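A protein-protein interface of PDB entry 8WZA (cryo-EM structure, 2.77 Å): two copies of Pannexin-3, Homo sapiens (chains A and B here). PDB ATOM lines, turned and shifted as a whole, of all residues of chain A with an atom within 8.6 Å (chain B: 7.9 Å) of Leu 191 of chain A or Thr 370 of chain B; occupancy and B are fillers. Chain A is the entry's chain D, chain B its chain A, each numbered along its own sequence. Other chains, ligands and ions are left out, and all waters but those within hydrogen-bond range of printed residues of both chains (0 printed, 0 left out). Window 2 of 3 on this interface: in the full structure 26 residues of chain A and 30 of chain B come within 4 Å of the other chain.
The backbone carbonyl oxygen of Tyr 195 of chain A sits at hydrogen-bond distance from the side-chain sulfur of Cys 198 of chain A (3.3 Å).
Of the 16 printed residues of chain A, 5 touch a printed residue of chain B.
Hydrophobic or aromatic side chains of chain A that line the printed part of chain B: Phe 142, Leu 191 and Tyr 195.
Along chain A the printed residues that touch a printed residue of chain B span positions 142 to 198.
Printed residues of chain B that touch a printed residue of chain A: Val 348, Cys 350, Val 351, Leu 352, Thr 370 and Ala 373.
Among the printed residues, 9 pairs touch across the chains.
Among the printed residues, no Asp or Glu carboxylate lies within 4 Å of a Lys or Arg side-chain nitrogen of the other chain.
Of the printed residues of chain B, Phe 142 of chain A touches Val 348 (3.6 Å).
Leu 191 of chain A touches just these residues of chain B: Thr 370 and Ala 373.
Printed residues of chain B within 4 Å of Tyr 195 of chain A: Cys 350 and Val 351.
Leu 196 of chain A touches none of the printed residues of chain B.
Of the printed residues of chain A, Val 351 of chain B touches Arg 194 (3.5 Å) and Tyr 195 (3.9 Å).
Val 365 of chain B touches none of the printed residues of chain A.
Of chain A, only Leu 191 (3.98 Å) and Arg 194 (2.4 Å) come within 4 Å of Thr 370 of chain B.
The nearest residue of chain B that does not touch Leu 191 of chain A is Gly 374 of chain B (4.3 Å).
The nearest residue of chain A that does not touch Thr 370 of chain B is Pro 190 of chain A (7.2 Å).
The backbone carbonyl oxygen of Val 351 of chain B lies within hydrogen-bond range of the guanidinium group of Arg 194 of chain A (3.5 Å).
The side-chain sulfur (SG) of Cys 198 of chain A is in hydrogen-bond range of the side-chain sulfur (SG) of Cys 350 of chain B, 3.5 Å away.
OG1 of Thr 370 of chain B lies close to NH2 of Arg 194 of chain A, 2.4 Å away.
No position is printed for both chains.
Of the 9 pairs that touch across the chains among the printed residues, none has its exchanged pair printed and touching as well.
Val 348 of chain B touches Phe 142 of chain A.
Thr 370 of chain B touches Leu 191 of chain A (CA to CD1, 3.98 Å).
Leu 191 of chain A touches Ala 373 of chain B.
Arg 194 of chain A touches Leu 352 of chain B (NH2 to CD2, 3.7 Å).
CE1 of Tyr 195 of chain A touches SG of Cys 350 of chain B, 3.8 Å away.
CA of Tyr 195 of chain A touches CG1 of Val 351 of chain B (3.9 Å).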
ATOM      1  N   PHE A 142     -36.416  21.538   9.562  1.00  0.00           N
ATOM      2  CA  PHE A 142     -35.215  21.104   8.851  1.00  0.00           C
ATOM      3  C   PHE A 142     -33.969  21.789   9.403  1.00  0.00           C
ATOM      4  O   PHE A 142     -32.943  21.138   9.646  1.00  0.00           O
ATOM      5  CB  PHE A 142     -35.349  21.372   7.353  1.00  0.00           C
ATOM      6  CG  PHE A 142     -34.074  21.148   6.588  1.00  0.00           C
ATOM      7  CD1 PHE A 142     -33.571  19.868   6.415  1.00  0.00           C
ATOM      8  CD2 PHE A 142     -33.370  22.215   6.056  1.00  0.00           C
ATOM      9  CE1 PHE A 142     -32.396  19.657   5.719  1.00  0.00           C
ATOM     10  CE2 PHE A 142     -32.193  22.009   5.358  1.00  0.00           C
ATOM     11  CZ  PHE A 142     -31.707  20.729   5.190  1.00  0.00           C
ATOM     12  N   GLU A 146     -30.776  20.081  11.350  1.00  0.00           N
ATOM     13  CA  GLU A 146     -29.412  20.209  10.849  1.00  0.00           C
ATOM     14  C   GLU A 146     -28.486  20.881  11.859  1.00  0.00           C
ATOM     15  O   GLU A 146     -27.299  20.544  11.924  1.00  0.00           O
ATOM     16  CB  GLU A 146     -29.409  20.986   9.532  1.00  0.00           C
ATOM     17  CG  GLU A 146     -28.082  20.949   8.794  1.00  0.00           C
ATOM     18  CD  GLU A 146     -27.998  19.797   7.813  1.00  0.00           C
ATOM     19  OE1 GLU A 146     -28.945  18.982   7.770  1.00  0.00           O
ATOM     20  OE2 GLU A 146     -26.987  19.704   7.085  1.00  0.00           O
ATOM     21  N   LYS A 149     -26.845  18.877  15.061  1.00  0.00           N
ATOM     22  CA  LYS A 149     -25.696  18.030  14.778  1.00  0.00           C
ATOM     23  C   LYS A 149     -24.369  18.756  14.959  1.00  0.00           C
ATOM     24  O   LYS A 149     -23.313  18.140  14.777  1.00  0.00           O
ATOM     25  CB  LYS A 149     -25.791  17.490  13.348  1.00  0.00           C
ATOM     26  CG  LYS A 149     -25.981  15.989  13.245  1.00  0.00           C
ATOM     27  CD  LYS A 149     -26.741  15.630  11.977  1.00  0.00           C
ATOM     28  CE  LYS A 149     -26.204  16.390  10.772  1.00  0.00           C
ATOM     29  NZ  LYS A 149     -26.902  16.013   9.513  1.00  0.00           N
ATOM     30  N   GLU A 188     -18.023  20.075   7.207  1.00  0.00           N
ATOM     31  CA  GLU A 188     -18.724  20.828   6.179  1.00  0.00           C
ATOM     32  C   GLU A 188     -20.202  20.459   6.156  1.00  0.00           C
ATOM     33  O   GLU A 188     -20.579  19.311   6.410  1.00  0.00           O
ATOM     34  CB  GLU A 188     -18.106  20.581   4.796  1.00  0.00           C
ATOM     35  CG  GLU A 188     -17.952  21.836   3.947  1.00  0.00           C
ATOM     36  CD  GLU A 188     -16.752  22.675   4.346  1.00  0.00           C
ATOM     37  OE1 GLU A 188     -16.039  22.293   5.299  1.00  0.00           O
ATOM     38  OE2 GLU A 188     -16.522  23.722   3.706  1.00  0.00           O
ATOM     39  N   PHE A 189     -21.033  21.453   5.846  1.00  0.00           N
ATOM     40  CA  PHE A 189     -22.481  21.285   5.718  1.00  0.00           C
ATOM     41  C   PHE A 189     -22.891  21.833   4.358  1.00  0.00           C
ATOM     42  O   PHE A 189     -23.321  22.989   4.243  1.00  0.00           O
ATOM     43  CB  PHE A 189     -23.229  21.991   6.850  1.00  0.00           C
ATOM     44  CG  PHE A 189     -22.989  21.391   8.206  1.00  0.00           C
ATOM     45  CD1 PHE A 189     -21.884  21.759   8.957  1.00  0.00           C
ATOM     46  CD2 PHE A 189     -23.870  20.462   8.734  1.00  0.00           C
ATOM     47  CE1 PHE A 189     -21.661  21.209  10.205  1.00  0.00           C
ATOM     48  CE2 PHE A 189     -23.653  19.909   9.982  1.00  0.00           C
ATOM     49  CZ  PHE A 189     -22.547  20.283  10.718  1.00  0.00           C
ATOM     50  N   PRO A 190     -22.770  21.028   3.301  1.00  0.00           N
ATOM     51  CA  PRO A 190     -23.027  21.544   1.949  1.00  0.00           C
ATOM     52  C   PRO A 190     -24.508  21.665   1.622  1.00  0.00           C
ATOM     53  O   PRO A 190     -24.901  22.520   0.822  1.00  0.00           O
ATOM     54  CB  PRO A 190     -22.333  20.520   1.038  1.00  0.00           C
ATOM     55  CG  PRO A 190     -21.960  19.345   1.918  1.00  0.00           C
ATOM     56  CD  PRO A 190     -22.469  19.589   3.303  1.00  0.00           C
ATOM     57  N   LEU A 191     -25.339  20.812   2.224  1.00  0.00           N
ATOM     58  CA  LEU A 191     -26.773  20.862   1.961  1.00  0.00           C
ATOM     59  C   LEU A 191     -27.429  22.061   2.638  1.00  0.00           C
ATOM     60  O   LEU A 191     -28.246  22.757   2.023  1.00  0.00           O
ATOM     61  CB  LEU A 191     -27.432  19.562   2.422  1.00  0.00           C
ATOM     62  CG  LEU A 191     -28.756  19.185   1.758  1.00  0.00           C
ATOM     63  CD1 LEU A 191     -28.509  18.612   0.371  1.00  0.00           C
ATOM     64  CD2 LEU A 191     -29.527  18.198   2.620  1.00  0.00           C
ATOM     65  N   LEU A 192     -27.077  22.317   3.902  1.00  0.00           N
ATOM     66  CA  LEU A 192     -27.658  23.442   4.629  1.00  0.00           C
ATOM     67  C   LEU A 192     -27.251  24.780   4.024  1.00  0.00           C
ATOM     68  O   LEU A 192     -28.069  25.708   3.975  1.00  0.00           O
ATOM     69  CB  LEU A 192     -27.255  23.376   6.103  1.00  0.00           C
ATOM     70  CG  LEU A 192     -27.611  24.591   6.960  1.00  0.00           C
ATOM     71  CD1 LEU A 192     -28.982  24.425   7.595  1.00  0.00           C
ATOM     72  CD2 LEU A 192     -26.550  24.822   8.024  1.00  0.00           C
ATOM     73  N   GLU A 193     -26.002  24.904   3.561  1.00  0.00           N
ATOM     74  CA  GLU A 193     -25.588  26.137   2.899  1.00  0.00           C
ATOM     75  C   GLU A 193     -26.427  26.391   1.660  1.00  0.00           C
ATOM     76  O   GLU A 193     -26.897  27.512   1.446  1.00  0.00           O
ATOM     77  CB  GLU A 193     -24.080  26.086   2.591  1.00  0.00           C
ATOM     78  CG  GLU A 193     -23.367  27.339   1.964  1.00  0.00           C
ATOM     79  CD  GLU A 193     -23.753  27.773   0.535  1.00  0.00           C
ATOM     80  OE1 GLU A 193     -24.650  27.213  -0.117  1.00  0.00           O
ATOM     81  OE2 GLU A 193     -23.143  28.755   0.065  1.00  0.00           O
ATOM     82  N   ARG A 194     -26.632  25.365   0.831  1.00  0.00           N
ATOM     83  CA  ARG A 194     -27.454  25.552  -0.359  1.00  0.00           C
ATOM     84  C   ARG A 194     -28.893  25.890   0.004  1.00  0.00           C
ATOM     85  O   ARG A 194     -29.516  26.732  -0.654  1.00  0.00           O
ATOM     86  CB  ARG A 194     -27.405  24.304  -1.237  1.00  0.00           C
ATOM     87  CG  ARG A 194     -27.579  24.587  -2.716  1.00  0.00           C
ATOM     88  CD  ARG A 194     -26.659  23.720  -3.552  1.00  0.00           C
ATOM     89  NE  ARG A 194     -27.253  22.418  -3.828  1.00  0.00           N
ATOM     90  CZ  ARG A 194     -27.884  22.106  -4.951  1.00  0.00           C
ATOM     91  NH1 ARG A 194     -28.032  22.986  -5.928  1.00  0.00           N
ATOM     92  NH2 ARG A 194     -28.383  20.881  -5.096  1.00  0.00           N
ATOM     93  N   TYR A 195     -29.430  25.249   1.045  1.00  0.00           N
ATOM     94  CA  TYR A 195     -30.774  25.573   1.509  1.00  0.00           C
ATOM     95  C   TYR A 195     -30.895  27.042   1.895  1.00  0.00           C
ATOM     96  O   TYR A 195     -31.826  27.727   1.453  1.00  0.00           O
ATOM     97  CB  TYR A 195     -31.135  24.676   2.693  1.00  0.00           C
ATOM     98  CG  TYR A 195     -32.613  24.566   2.974  1.00  0.00           C
ATOM     99  CD1 TYR A 195     -33.390  23.610   2.333  1.00  0.00           C
ATOM    100  CD2 TYR A 195     -33.230  25.407   3.888  1.00  0.00           C
ATOM    101  CE1 TYR A 195     -34.741  23.502   2.588  1.00  0.00           C
ATOM    102  CE2 TYR A 195     -34.581  25.306   4.152  1.00  0.00           C
ATOM    103  CZ  TYR A 195     -35.332  24.352   3.498  1.00  0.00           C
ATOM    104  OH  TYR A 195     -36.678  24.246   3.757  1.00  0.00           O
ATOM    105  N   LEU A 196     -29.957  27.547   2.698  1.00  0.00           N
ATOM    106  CA  LEU A 196     -29.964  28.949   3.098  1.00  0.00           C
ATOM    107  C   LEU A 196     -29.755  29.901   1.928  1.00  0.00           C
ATOM    108  O   LEU A 196     -30.413  30.946   1.865  1.00  0.00           O
ATOM    109  CB  LEU A 196     -28.891  29.199   4.161  1.00  0.00           C
ATOM    110  CG  LEU A 196     -29.059  28.413   5.463  1.00  0.00           C
ATOM    111  CD1 LEU A 196     -27.937  28.731   6.436  1.00  0.00           C
ATOM    112  CD2 LEU A 196     -30.416  28.694   6.088  1.00  0.00           C
ATOM    113  N   ALA A 197     -28.854  29.566   1.002  1.00  0.00           N
ATOM    114  CA  ALA A 197     -28.629  30.418  -0.160  1.00  0.00           C
ATOM    115  C   ALA A 197     -29.878  30.507  -1.028  1.00  0.00           C
ATOM    116  O   ALA A 197     -30.214  31.584  -1.533  1.00  0.00           O
ATOM    117  CB  ALA A 197     -27.445  29.897  -0.974  1.00  0.00           C
ATOM    118  N   CYS A 198     -30.574  29.383  -1.216  1.00  0.00           N
ATOM    119  CA  CYS A 198     -31.807  29.403  -1.993  1.00  0.00           C
ATOM    120  C   CYS A 198     -32.918  30.154  -1.272  1.00  0.00           C
ATOM    121  O   CYS A 198     -33.697  30.867  -1.912  1.00  0.00           O
ATOM    122  CB  CYS A 198     -32.254  27.975  -2.306  1.00  0.00           C
ATOM    123  SG  CYS A 198     -33.591  27.371  -1.253  1.00  0.00           S
ATOM    124  N   LEU A 313     -22.423  29.435   8.971  1.00  0.00           N
ATOM    125  CA  LEU A 313     -23.194  29.715   7.764  1.00  0.00           C
ATOM    126  C   LEU A 313     -24.323  30.702   8.028  1.00  0.00           C
ATOM    127  O   LEU A 313     -24.666  31.497   7.146  1.00  0.00           O
ATOM    128  CB  LEU A 313     -23.748  28.413   7.185  1.00  0.00           C
ATOM    129  CG  LEU A 313     -22.719  27.309   6.934  1.00  0.00           C
ATOM    130  CD1 LEU A 313     -23.399  26.028   6.477  1.00  0.00           C
ATOM    131  CD2 LEU A 313     -21.683  27.763   5.919  1.00  0.00           C
ATOM    132  N   LYS A 317     -24.173  34.646   5.743  1.00  0.00           N
ATOM    133  CA  LYS A 317     -25.139  35.184   4.785  1.00  0.00           C
ATOM    134  C   LYS A 317     -25.933  36.324   5.425  1.00  0.00           C
ATOM    135  O   LYS A 317     -27.138  36.240   5.666  1.00  0.00           O
ATOM    136  CB  LYS A 317     -26.057  34.077   4.280  1.00  0.00           C
ATOM    137  CG  LYS A 317     -25.399  32.710   4.223  1.00  0.00           C
ATOM    138  CD  LYS A 317     -26.307  31.690   3.557  1.00  0.00           C
ATOM    139  CE  LYS A 317     -25.512  30.723   2.700  1.00  0.00           C
ATOM    140  NZ  LYS A 317     -24.926  31.396   1.509  1.00  0.00           N
ATOM    141  N   ILE B 155     -32.043   5.829  -3.074  1.00  0.00           N
ATOM    142  CA  ILE B 155     -30.807   6.044  -2.345  1.00  0.00           C
ATOM    143  C   ILE B 155     -30.199   4.736  -1.844  1.00  0.00           C
ATOM    144  O   ILE B 155     -28.970   4.629  -1.770  1.00  0.00           O
ATOM    145  CB  ILE B 155     -31.020   7.033  -1.178  1.00  0.00           C
ATOM    146  CG1 ILE B 155     -29.689   7.377  -0.505  1.00  0.00           C
ATOM    147  CG2 ILE B 155     -32.013   6.475  -0.166  1.00  0.00           C
ATOM    148  CD1 ILE B 155     -28.644   7.916  -1.458  1.00  0.00           C
ATOM    149  N   TRP B 345     -37.037  14.781   2.890  1.00  0.00           N
ATOM    150  CA  TRP B 345     -36.290  15.004   1.656  1.00  0.00           C
ATOM    151  C   TRP B 345     -37.154  15.523   0.510  1.00  0.00           C
ATOM    152  O   TRP B 345     -36.737  16.432  -0.213  1.00  0.00           O
ATOM    153  CB  TRP B 345     -35.628  13.691   1.224  1.00  0.00           C
ATOM    154  CG  TRP B 345     -36.621  12.555   1.101  1.00  0.00           C
ATOM    155  CD1 TRP B 345     -37.239  11.889   2.122  1.00  0.00           C
ATOM    156  CD2 TRP B 345     -37.128  11.981  -0.111  1.00  0.00           C
ATOM    157  NE1 TRP B 345     -38.087  10.932   1.623  1.00  0.00           N
ATOM    158  CE2 TRP B 345     -38.038  10.967   0.254  1.00  0.00           C
ATOM    159  CE3 TRP B 345     -36.897  12.221  -1.469  1.00  0.00           C
ATOM    160  CZ2 TRP B 345     -38.714  10.196  -0.687  1.00  0.00           C
ATOM    161  CZ3 TRP B 345     -37.570  11.452  -2.402  1.00  0.00           C
ATOM    162  CH2 TRP B 345     -38.467  10.452  -2.007  1.00  0.00           C
ATOM    163  N   VAL B 348     -37.671  18.898   1.407  1.00  0.00           N
ATOM    164  CA  VAL B 348     -36.340  19.493   1.435  1.00  0.00           C
ATOM    165  C   VAL B 348     -35.756  19.624   0.034  1.00  0.00           C
ATOM    166  O   VAL B 348     -34.846  20.433  -0.182  1.00  0.00           O
ATOM    167  CB  VAL B 348     -35.413  18.670   2.352  1.00  0.00           C
ATOM    168  CG1 VAL B 348     -34.097  19.395   2.589  1.00  0.00           C
ATOM    169  CG2 VAL B 348     -36.102  18.381   3.675  1.00  0.00           C
ATOM    170  N   LEU B 349     -36.274  18.874  -0.938  1.00  0.00           N
ATOM    171  CA  LEU B 349     -35.792  18.999  -2.308  1.00  0.00           C
ATOM    172  C   LEU B 349     -36.334  20.271  -2.946  1.00  0.00           C
ATOM    173  O   LEU B 349     -36.992  20.223  -3.989  1.00  0.00           O
ATOM    174  CB  LEU B 349     -36.189  17.777  -3.140  1.00  0.00           C
ATOM    175  CG  LEU B 349     -35.282  16.548  -3.056  1.00  0.00           C
ATOM    176  CD1 LEU B 349     -36.048  15.289  -3.425  1.00  0.00           C
ATOM    177  CD2 LEU B 349     -34.072  16.719  -3.958  1.00  0.00           C
ATOM    178  N   CYS B 350     -36.056  21.414  -2.318  1.00  0.00           N
ATOM    179  CA  CYS B 350     -36.361  22.722  -2.877  1.00  0.00           C
ATOM    180  C   CYS B 350     -35.137  23.393  -3.479  1.00  0.00           C
ATOM    181  O   CYS B 350     -35.276  24.424  -4.146  1.00  0.00           O
ATOM    182  CB  CYS B 350     -36.973  23.631  -1.803  1.00  0.00           C
ATOM    183  SG  CYS B 350     -35.770  24.607  -0.875  1.00  0.00           S
ATOM    184  N   VAL B 351     -33.944  22.831  -3.258  1.00  0.00           N
ATOM    185  CA  VAL B 351     -32.726  23.318  -3.902  1.00  0.00           C
ATOM    186  C   VAL B 351     -32.520  22.715  -5.278  1.00  0.00           C
ATOM    187  O   VAL B 351     -31.525  23.035  -5.943  1.00  0.00           O
ATOM    188  CB  VAL B 351     -31.494  23.024  -3.023  1.00  0.00           C
ATOM    189  CG1 VAL B 351     -31.736  23.498  -1.598  1.00  0.00           C
ATOM    190  CG2 VAL B 351     -31.175  21.536  -3.042  1.00  0.00           C
ATOM    191  N   LEU B 352     -33.427  21.850  -5.729  1.00  0.00           N
ATOM    192  CA  LEU B 352     -33.332  21.189  -7.025  1.00  0.00           C
ATOM    193  C   LEU B 352     -34.378  21.726  -7.999  1.00  0.00           C
ATOM    194  O   LEU B 352     -34.933  20.987  -8.814  1.00  0.00           O
ATOM    195  CB  LEU B 352     -33.469  19.677  -6.867  1.00  0.00           C
ATOM    196  CG  LEU B 352     -32.413  18.814  -7.563  1.00  0.00           C
ATOM    197  CD1 LEU B 352     -32.578  18.857  -9.073  1.00  0.00           C
ATOM    198  CD2 LEU B 352     -31.015  19.261  -7.162  1.00  0.00           C
ATOM    199  N   VAL B 365     -26.529  16.951 -14.252  1.00  0.00           N
ATOM    200  CA  VAL B 365     -25.386  17.102 -13.360  1.00  0.00           C
ATOM    201  C   VAL B 365     -25.728  17.845 -12.068  1.00  0.00           C
ATOM    202  O   VAL B 365     -24.934  17.801 -11.116  1.00  0.00           O
ATOM    203  CB  VAL B 365     -24.225  17.810 -14.093  1.00  0.00           C
ATOM    204  CG1 VAL B 365     -22.894  17.535 -13.404  1.00  0.00           C
ATOM    205  CG2 VAL B 365     -24.177  17.375 -15.550  1.00  0.00           C
ATOM    206  N   VAL B 366     -26.885  18.512 -11.998  1.00  0.00           N
ATOM    207  CA  VAL B 366     -27.196  19.309 -10.812  1.00  0.00           C
ATOM    208  C   VAL B 366     -27.407  18.428  -9.585  1.00  0.00           C
ATOM    209  O   VAL B 366     -27.097  18.838  -8.460  1.00  0.00           O
ATOM    210  CB  VAL B 366     -28.416  20.214 -11.083  1.00  0.00           C
ATOM    211  CG1 VAL B 366     -29.688  19.391 -11.223  1.00  0.00           C
ATOM    212  CG2 VAL B 366     -28.565  21.257  -9.983  1.00  0.00           C
ATOM    213  N   ASP B 367     -27.921  17.211  -9.770  1.00  0.00           N
ATOM    214  CA  ASP B 367     -28.247  16.327  -8.658  1.00  0.00           C
ATOM    215  C   ASP B 367     -27.041  15.542  -8.153  1.00  0.00           C
ATOM    216  O   ASP B 367     -27.215  14.540  -7.449  1.00  0.00           O
ATOM    217  CB  ASP B 367     -29.364  15.362  -9.061  1.00  0.00           C
ATOM    218  CG  ASP B 367     -28.902  14.324 -10.062  1.00  0.00           C
ATOM    219  OD1 ASP B 367     -28.184  14.694 -11.014  1.00  0.00           O
ATOM    220  OD2 ASP B 367     -29.252  13.136  -9.896  1.00  0.00           O
ATOM    221  N   PHE B 368     -25.827  15.972  -8.496  1.00  0.00           N
ATOM    222  CA  PHE B 368     -24.624  15.276  -8.062  1.00  0.00           C
ATOM    223  C   PHE B 368     -24.378  15.399  -6.563  1.00  0.00           C
ATOM    224  O   PHE B 368     -23.590  14.620  -6.016  1.00  0.00           O
ATOM    225  CB  PHE B 368     -23.412  15.810  -8.831  1.00  0.00           C
ATOM    226  CG  PHE B 368     -22.365  14.773  -9.119  1.00  0.00           C
ATOM    227  CD1 PHE B 368     -22.470  13.956 -10.233  1.00  0.00           C
ATOM    228  CD2 PHE B 368     -21.273  14.618  -8.281  1.00  0.00           C
ATOM    229  CE1 PHE B 368     -21.507  13.005 -10.507  1.00  0.00           C
ATOM    230  CE2 PHE B 368     -20.306  13.666  -8.549  1.00  0.00           C
ATOM    231  CZ  PHE B 368     -20.424  12.859  -9.663  1.00  0.00           C
ATOM    232  N   MET B 369     -25.015  16.360  -5.893  1.00  0.00           N
ATOM    233  CA  MET B 369     -24.838  16.572  -4.460  1.00  0.00           C
ATOM    234  C   MET B 369     -26.055  16.180  -3.635  1.00  0.00           C
ATOM    235  O   MET B 369     -25.921  15.477  -2.630  1.00  0.00           O
ATOM    236  CB  MET B 369     -24.502  18.046  -4.160  1.00  0.00           C
ATOM    237  CG  MET B 369     -23.088  18.527  -4.488  1.00  0.00           C
ATOM    238  SD  MET B 369     -22.312  17.861  -5.969  1.00  0.00           S
ATOM    239  CE  MET B 369     -23.068  18.904  -7.217  1.00  0.00           C
ATOM    240  N   THR B 370     -27.248  16.620  -4.043  1.00  0.00           N
ATOM    241  CA  THR B 370     -28.376  16.713  -3.119  1.00  0.00           C
ATOM    242  C   THR B 370     -28.911  15.341  -2.715  1.00  0.00           C
ATOM    243  O   THR B 370     -29.159  15.088  -1.529  1.00  0.00           O
ATOM    244  CB  THR B 370     -29.489  17.556  -3.744  1.00  0.00           C
ATOM    245  OG1 THR B 370     -29.030  18.903  -3.912  1.00  0.00           O
ATOM    246  CG2 THR B 370     -30.719  17.560  -2.854  1.00  0.00           C
ATOM    247  N   LEU B 371     -29.116  14.447  -3.688  1.00  0.00           N
ATOM    248  CA  LEU B 371     -29.846  13.212  -3.409  1.00  0.00           C
ATOM    249  C   LEU B 371     -29.110  12.334  -2.403  1.00  0.00           C
ATOM    250  O   LEU B 371     -29.724  11.798  -1.473  1.00  0.00           O
ATOM    251  CB  LEU B 371     -30.099  12.444  -4.707  1.00  0.00           C
ATOM    252  CG  LEU B 371     -31.086  11.278  -4.604  1.00  0.00           C
ATOM    253  CD1 LEU B 371     -32.311  11.673  -3.792  1.00  0.00           C
ATOM    254  CD2 LEU B 371     -31.493  10.793  -5.986  1.00  0.00           C
ATOM    255  N   LEU B 372     -27.796  12.175  -2.569  1.00  0.00           N
ATOM    256  CA  LEU B 372     -27.032  11.357  -1.634  1.00  0.00           C
ATOM    257  C   LEU B 372     -26.804  12.060  -0.303  1.00  0.00           C
ATOM    258  O   LEU B 372     -26.662  11.385   0.722  1.00  0.00           O
ATOM    259  CB  LEU B 372     -25.690  10.962  -2.252  1.00  0.00           C
ATOM    260  CG  LEU B 372     -24.713  12.099  -2.554  1.00  0.00           C
ATOM    261  CD1 LEU B 372     -23.284  11.675  -2.253  1.00  0.00           C
ATOM    262  CD2 LEU B 372     -24.852  12.546  -3.998  1.00  0.00           C
ATOM    263  N   ALA B 373     -26.766  13.394  -0.293  1.00  0.00           N
ATOM    264  CA  ALA B 373     -26.572  14.144   0.940  1.00  0.00           C
ATOM    265  C   ALA B 373     -27.850  14.287   1.754  1.00  0.00           C
ATOM    266  O   ALA B 373     -27.776  14.660   2.931  1.00  0.00           O
ATOM    267  CB  ALA B 373     -26.003  15.530   0.631  1.00  0.00           C
ATOM    268  N   GLY B 374     -29.006  13.998   1.168  1.00  0.00           N
ATOM    269  CA  GLY B 374     -30.273  14.070   1.862  1.00  0.00           C
ATOM    270  C   GLY B 374     -30.598  12.866   2.718  1.00  0.00           C
ATOM    271  O   GLY B 374     -31.737  12.738   3.178  1.00  0.00           O
ATOM    272  N   LEU B 375     -29.632  11.978   2.941  1.00  0.00           N
ATOM    273  CA  LEU B 375     -29.866  10.787   3.744  1.00  0.00           C
ATOM    274  C   LEU B 375     -30.172  11.161   5.190  1.00  0.00           C
ATOM    275  O   LEU B 375     -29.730  12.197   5.697  1.00  0.00           O
ATOM    276  CB  LEU B 375     -28.649   9.859   3.684  1.00  0.00           C
ATOM    277  CG  LEU B 375     -27.439  10.196   4.563  1.00  0.00           C
ATOM    278  CD1 LEU B 375     -26.551   8.973   4.732  1.00  0.00           C
ATOM    279  CD2 LEU B 375     -26.639  11.363   4.000  1.00  0.00           C
